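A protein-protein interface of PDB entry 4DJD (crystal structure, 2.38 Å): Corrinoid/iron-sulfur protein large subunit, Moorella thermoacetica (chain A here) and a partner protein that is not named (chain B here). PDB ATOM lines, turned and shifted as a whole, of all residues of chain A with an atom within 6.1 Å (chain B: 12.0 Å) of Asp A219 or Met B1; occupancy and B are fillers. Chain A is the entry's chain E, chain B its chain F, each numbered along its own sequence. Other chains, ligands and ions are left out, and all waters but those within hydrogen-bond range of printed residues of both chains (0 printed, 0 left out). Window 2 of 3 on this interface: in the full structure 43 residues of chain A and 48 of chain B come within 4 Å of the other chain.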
ATOM      1  N   GLU A 212      19.339 -21.728  12.731  1.00  0.00           N
ATOM      2  CA  GLU A 212      18.076 -21.437  12.052  1.00  0.00           C
ATOM      3  C   GLU A 212      16.959 -21.034  13.021  1.00  0.00           C
ATOM      4  O   GLU A 212      16.285 -20.027  12.806  1.00  0.00           O
ATOM      5  CB  GLU A 212      17.641 -22.633  11.198  1.00  0.00           C
ATOM      6  CG  GLU A 212      16.256 -22.501  10.598  1.00  0.00           C
ATOM      7  CD  GLU A 212      16.163 -21.387   9.574  1.00  0.00           C
ATOM      8  OE1 GLU A 212      17.200 -21.059   8.954  1.00  0.00           O
ATOM      9  OE2 GLU A 212      15.051 -20.841   9.393  1.00  0.00           O
ATOM     10  N   LEU A 214      17.376 -19.995  16.102  1.00  0.00           N
ATOM     11  CA  LEU A 214      17.851 -18.765  16.727  1.00  0.00           C
ATOM     12  C   LEU A 214      17.431 -17.544  15.926  1.00  0.00           C
ATOM     13  O   LEU A 214      16.825 -16.617  16.464  1.00  0.00           O
ATOM     14  CB  LEU A 214      19.373 -18.779  16.847  1.00  0.00           C
ATOM     15  CG  LEU A 214      19.981 -17.492  17.409  1.00  0.00           C
ATOM     16  CD1 LEU A 214      19.392 -17.208  18.781  1.00  0.00           C
ATOM     17  CD2 LEU A 214      21.507 -17.586  17.480  1.00  0.00           C
ATOM     18  N   ALA A 215      17.753 -17.563  14.634  1.00  0.00           N
ATOM     19  CA  ALA A 215      17.473 -16.443  13.742  1.00  0.00           C
ATOM     20  C   ALA A 215      15.980 -16.140  13.623  1.00  0.00           C
ATOM     21  O   ALA A 215      15.582 -14.973  13.633  1.00  0.00           O
ATOM     22  CB  ALA A 215      18.073 -16.697  12.375  1.00  0.00           C
ATOM     23  N   GLU A 216      15.161 -17.185  13.507  1.00  0.00           N
ATOM     24  CA  GLU A 216      13.705 -17.021  13.422  1.00  0.00           C
ATOM     25  C   GLU A 216      13.123 -16.399  14.688  1.00  0.00           C
ATOM     26  O   GLU A 216      12.254 -15.532  14.617  1.00  0.00           O
ATOM     27  CB  GLU A 216      13.016 -18.362  13.155  1.00  0.00           C
ATOM     28  CG  GLU A 216      13.278 -18.949  11.779  1.00  0.00           C
ATOM     29  CD  GLU A 216      12.718 -20.354  11.633  1.00  0.00           C
ATOM     30  OE1 GLU A 216      12.575 -21.045  12.666  1.00  0.00           O
ATOM     31  OE2 GLU A 216      12.418 -20.765  10.490  1.00  0.00           O
ATOM     32  N   LEU A 217      13.609 -16.843  15.844  1.00  0.00           N
ATOM     33  CA  LEU A 217      13.096 -16.359  17.120  1.00  0.00           C
ATOM     34  C   LEU A 217      13.478 -14.899  17.346  1.00  0.00           C
ATOM     35  O   LEU A 217      12.659 -14.104  17.808  1.00  0.00           O
ATOM     36  CB  LEU A 217      13.604 -17.222  18.276  1.00  0.00           C
ATOM     37  CG  LEU A 217      12.588 -17.599  19.359  1.00  0.00           C
ATOM     38  CD1 LEU A 217      13.293 -17.943  20.661  1.00  0.00           C
ATOM     39  CD2 LEU A 217      11.555 -16.512  19.583  1.00  0.00           C
ATOM     40  N   VAL A 218      14.721 -14.552  17.024  1.00  0.00           N
ATOM     41  CA  VAL A 218      15.174 -13.169  17.124  1.00  0.00           C
ATOM     42  C   VAL A 218      14.276 -12.234  16.320  1.00  0.00           C
ATOM     43  O   VAL A 218      13.869 -11.180  16.813  1.00  0.00           O
ATOM     44  CB  VAL A 218      16.634 -13.006  16.653  1.00  0.00           C
ATOM     45  CG1 VAL A 218      17.007 -11.530  16.555  1.00  0.00           C
ATOM     46  CG2 VAL A 218      17.572 -13.731  17.592  1.00  0.00           C
ATOM     47  N   ASP A 219      13.957 -12.633  15.089  1.00  0.00           N
ATOM     48  CA  ASP A 219      13.101 -11.827  14.219  1.00  0.00           C
ATOM     49  C   ASP A 219      11.710 -11.586  14.815  1.00  0.00           C
ATOM     50  O   ASP A 219      11.135 -10.510  14.643  1.00  0.00           O
ATOM     51  CB  ASP A 219      12.985 -12.449  12.823  1.00  0.00           C
ATOM     52  CG  ASP A 219      14.278 -12.360  12.036  1.00  0.00           C
ATOM     53  OD1 ASP A 219      15.123 -11.505  12.372  1.00  0.00           O
ATOM     54  OD2 ASP A 219      14.452 -13.143  11.079  1.00  0.00           O
ATOM     55  N   LYS A 220      11.172 -12.583  15.512  1.00  0.00           N
ATOM     56  CA  LYS A 220       9.891 -12.418  16.192  1.00  0.00           C
ATOM     57  C   LYS A 220      10.006 -11.439  17.356  1.00  0.00           C
ATOM     58  O   LYS A 220       9.153 -10.575  17.534  1.00  0.00           O
ATOM     59  CB  LYS A 220       9.352 -13.764  16.680  1.00  0.00           C
ATOM     60  CG  LYS A 220       9.018 -14.724  15.558  1.00  0.00           C
ATOM     61  CD  LYS A 220       8.411 -16.015  16.076  1.00  0.00           C
ATOM     62  CE  LYS A 220       8.115 -16.964  14.924  1.00  0.00           C
ATOM     63  NZ  LYS A 220       7.499 -18.240  15.380  1.00  0.00           N
ATOM     64  N   ILE A 221      11.074 -11.569  18.137  1.00  0.00           N
ATOM     65  CA  ILE A 221      11.268 -10.725  19.312  1.00  0.00           C
ATOM     66  C   ILE A 221      11.512  -9.260  18.941  1.00  0.00           C
ATOM     67  O   ILE A 221      10.962  -8.355  19.572  1.00  0.00           O
ATOM     68  CB  ILE A 221      12.394 -11.271  20.228  1.00  0.00           C
ATOM     69  CG1 ILE A 221      12.036 -12.680  20.708  1.00  0.00           C
ATOM     70  CG2 ILE A 221      12.614 -10.353  21.425  1.00  0.00           C
ATOM     71  CD1 ILE A 221      13.037 -13.282  21.661  1.00  0.00           C
ATOM     72  N   VAL A 222      12.314  -9.026  17.903  1.00  0.00           N
ATOM     73  CA  VAL A 222      12.567  -7.661  17.450  1.00  0.00           C
ATOM     74  C   VAL A 222      11.291  -7.046  16.868  1.00  0.00           C
ATOM     75  O   VAL A 222      11.056  -5.844  16.997  1.00  0.00           O
ATOM     76  CB  VAL A 222      13.739  -7.579  16.436  1.00  0.00           C
ATOM     77  CG1 VAL A 222      13.456  -8.420  15.222  1.00  0.00           C
ATOM     78  CG2 VAL A 222      13.994  -6.137  16.017  1.00  0.00           C
ATOM     79  N   ALA A 223      10.455  -7.880  16.257  1.00  0.00           N
ATOM     80  CA  ALA A 223       9.178  -7.418  15.727  1.00  0.00           C
ATOM     81  C   ALA A 223       8.226  -7.039  16.859  1.00  0.00           C
ATOM     82  O   ALA A 223       7.307  -6.249  16.659  1.00  0.00           O
ATOM     83  CB  ALA A 223       8.552  -8.474  14.831  1.00  0.00           C
ATOM     84  N   LEU A 224       8.447  -7.605  18.044  1.00  0.00           N
ATOM     85  CA  LEU A 224       7.650  -7.248  19.215  1.00  0.00           C
ATOM     86  C   LEU A 224       8.198  -5.993  19.891  1.00  0.00           C
ATOM     87  O   LEU A 224       7.622  -5.497  20.855  1.00  0.00           O
ATOM     88  CB  LEU A 224       7.580  -8.408  20.215  1.00  0.00           C
ATOM     89  CG  LEU A 224       6.870  -9.685  19.754  1.00  0.00           C
ATOM     90  CD1 LEU A 224       6.935 -10.764  20.830  1.00  0.00           C
ATOM     91  CD2 LEU A 224       5.424  -9.400  19.365  1.00  0.00           C
ATOM     92  N   PHE A 257      23.824  -9.388   8.600  1.00  0.00           N
ATOM     93  CA  PHE A 257      22.659 -10.205   8.922  1.00  0.00           C
ATOM     94  C   PHE A 257      22.112  -9.797  10.287  1.00  0.00           C
ATOM     95  O   PHE A 257      22.630 -10.221  11.321  1.00  0.00           O
ATOM     96  CB  PHE A 257      23.049 -11.684   8.917  1.00  0.00           C
ATOM     97  CG  PHE A 257      21.894 -12.620   9.112  1.00  0.00           C
ATOM     98  CD1 PHE A 257      20.838 -12.635   8.214  1.00  0.00           C
ATOM     99  CD2 PHE A 257      21.872 -13.500  10.180  1.00  0.00           C
ATOM    100  CE1 PHE A 257      19.772 -13.502   8.388  1.00  0.00           C
ATOM    101  CE2 PHE A 257      20.806 -14.373  10.362  1.00  0.00           C
ATOM    102  CZ  PHE A 257      19.757 -14.372   9.466  1.00  0.00           C
ATOM    103  N   ARG A 258      21.062  -8.980  10.280  1.00  0.00           N
ATOM    104  CA  ARG A 258      20.575  -8.313  11.490  1.00  0.00           C
ATOM    105  C   ARG A 258      20.116  -9.243  12.613  1.00  0.00           C
ATOM    106  O   ARG A 258      20.150  -8.866  13.784  1.00  0.00           O
ATOM    107  CB  ARG A 258      19.459  -7.322  11.151  1.00  0.00           C
ATOM    108  CG  ARG A 258      19.879  -6.214  10.201  1.00  0.00           C
ATOM    109  CD  ARG A 258      19.137  -4.925  10.515  1.00  0.00           C
ATOM    110  NE  ARG A 258      17.686  -5.090  10.480  1.00  0.00           N
ATOM    111  CZ  ARG A 258      16.823  -4.231  11.017  1.00  0.00           C
ATOM    112  NH1 ARG A 258      17.267  -3.148  11.639  1.00  0.00           N
ATOM    113  NH2 ARG A 258      15.519  -4.459  10.941  1.00  0.00           N
ATOM    114  N   SER A 259      19.689 -10.449  12.261  1.00  0.00           N
ATOM    115  CA  SER A 259      19.228 -11.411  13.260  1.00  0.00           C
ATOM    116  C   SER A 259      20.351 -11.838  14.204  1.00  0.00           C
ATOM    117  O   SER A 259      20.096 -12.334  15.303  1.00  0.00           O
ATOM    118  CB  SER A 259      18.637 -12.645  12.576  1.00  0.00           C
ATOM    119  OG  SER A 259      17.657 -12.277  11.626  1.00  0.00           O
ATOM    120  N   MET B   1      13.144 -17.601   8.026  1.00  0.00           N
ATOM    121  CA  MET B   1      14.451 -16.948   8.018  1.00  0.00           C
ATOM    122  C   MET B   1      15.558 -17.932   7.640  1.00  0.00           C
ATOM    123  O   MET B   1      16.235 -18.486   8.508  1.00  0.00           O
ATOM    124  CB  MET B   1      14.737 -16.295   9.376  1.00  0.00           C
ATOM    125  CG  MET B   1      16.082 -15.579   9.470  1.00  0.00           C
ATOM    126  SD  MET B   1      16.506 -14.638   7.989  1.00  0.00           S
ATOM    127  CE  MET B   1      15.245 -13.366   7.994  1.00  0.00           C
ATOM    128  N   ALA B   2      15.732 -18.144   6.338  1.00  0.00           N
ATOM    129  CA  ALA B   2      16.748 -19.063   5.838  1.00  0.00           C
ATOM    130  C   ALA B   2      18.151 -18.540   6.128  1.00  0.00           C
ATOM    131  O   ALA B   2      18.537 -17.471   5.655  1.00  0.00           O
ATOM    132  CB  ALA B   2      16.563 -19.298   4.346  1.00  0.00           C
ATOM    133  N   VAL B   3      18.906 -19.296   6.918  1.00  0.00           N
ATOM    134  CA  VAL B   3      20.268 -18.915   7.263  1.00  0.00           C
ATOM    135  C   VAL B   3      21.258 -19.597   6.326  1.00  0.00           C
ATOM    136  O   VAL B   3      21.193 -20.807   6.107  1.00  0.00           O
ATOM    137  CB  VAL B   3      20.594 -19.260   8.730  1.00  0.00           C
ATOM    138  CG1 VAL B   3      22.078 -19.075   9.020  1.00  0.00           C
ATOM    139  CG2 VAL B   3      19.753 -18.410   9.665  1.00  0.00           C
ATOM    140  N   GLN B   4      22.157 -18.807   5.753  1.00  0.00           N
ATOM    141  CA  GLN B   4      23.191 -19.331   4.875  1.00  0.00           C
ATOM    142  C   GLN B   4      24.529 -19.261   5.596  1.00  0.00           C
ATOM    143  O   GLN B   4      24.985 -18.183   5.975  1.00  0.00           O
ATOM    144  CB  GLN B   4      23.250 -18.535   3.568  1.00  0.00           C
ATOM    145  CG  GLN B   4      24.507 -18.788   2.729  1.00  0.00           C
ATOM    146  CD  GLN B   4      24.576 -20.199   2.158  1.00  0.00           C
ATOM    147  OE1 GLN B   4      23.599 -20.709   1.605  1.00  0.00           O
ATOM    148  NE2 GLN B   4      25.738 -20.838   2.293  1.00  0.00           N
ATOM    149  N   ILE B   5      25.158 -20.409   5.801  1.00  0.00           N
ATOM    150  CA  ILE B   5      26.441 -20.401   6.482  1.00  0.00           C
ATOM    151  C   ILE B   5      27.523 -19.847   5.558  1.00  0.00           C
ATOM    152  O   ILE B   5      27.512 -20.081   4.348  1.00  0.00           O
ATOM    153  CB  ILE B   5      26.834 -21.791   7.049  1.00  0.00           C
ATOM    154  CG1 ILE B   5      27.915 -22.444   6.199  1.00  0.00           C
ATOM    155  CG2 ILE B   5      25.616 -22.694   7.191  1.00  0.00           C
ATOM    156  CD1 ILE B   5      28.835 -23.316   6.993  1.00  0.00           C
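OE1 of Glu A212 touches CA of Ala B2, at 3.7 Å. Ala A215 touches Met B1 (CB to CG, 3.7 Å). Val B3 touches Ala A215. Met B1 touches Glu A216. Asp A219 touches Met B1 (OD2 to CE, 3.2 Å). SD of Met B1 touches CE1 of Phe A257 (3.5 Å).
The side-chain carboxylate of Glu A212 lies within hydrogen-bond range of the backbone NH of Val B3, 3.2 Å away. The side-chain carboxylate of Glu A212 lies close to the backbone carbonyl oxygen of Met B1 (2.8 Å).
The side-chain carboxylate of Asp A219 sits at hydrogen-bond distance from the side-chain hydroxyl of Ser A259 (2.8 Å).
Ala A215 touches just these residues of chain B: Met B1 and Val B3. Of chain B, only Met B1 (3.9 Å) comes within 4 Å of Glu A216. No residue of chain B comes within 4 Å of Val A218. Of chain B, only Met B1 comes within 4 Å of Asp A219. No residue of chain B comes within 4 Å of Lys A220. No residue of chain B comes within 4 Å of Ile A221. No residue of chain B comes within 4 Å of Val A222. Ala A223 touches none of the printed residues of chain B. Printed residues of chain B within 4 Å of Phe A257: Met B1. No residue of chain B comes within 4 Å of Ser A259. Of chain A, only Glu A212 (2.8 Å), Ala A215 (3.7 Å), Glu A216 (3.9 Å), Asp A219 (3.2 Å) and Phe A257 (3.5 Å) come within 4 Å of Met B1. Printed residues of chain A within 4 Å of Ala B2: Glu A212 (3.7 Å). Of the printed residues of chain A, Val B3 touches Glu A212 (3.2 Å) and Ala A215 (3.6 Å). Gln B4 touches none of the printed residues of chain A. The nearest residue of chain B that does not touch Asp A219 is Ala B2 (7.0 Å).
Of the 15 printed residues of chain A, 5 touch a printed residue of chain B. Hydrophobic or aromatic side chains of chain A that line the printed part of chain B: Ala A215 and Phe A257. Hydrophobic or aromatic side chains of chain B within 4 Å of the printed part of chain A: Met B1 and Val B3. Among the printed residues, 8 pairs touch across the chains. Among the printed residues, no Asp or Glu carboxylate lies within 4 Å of a Lys or Arg side-chain nitrogen of the other chain.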
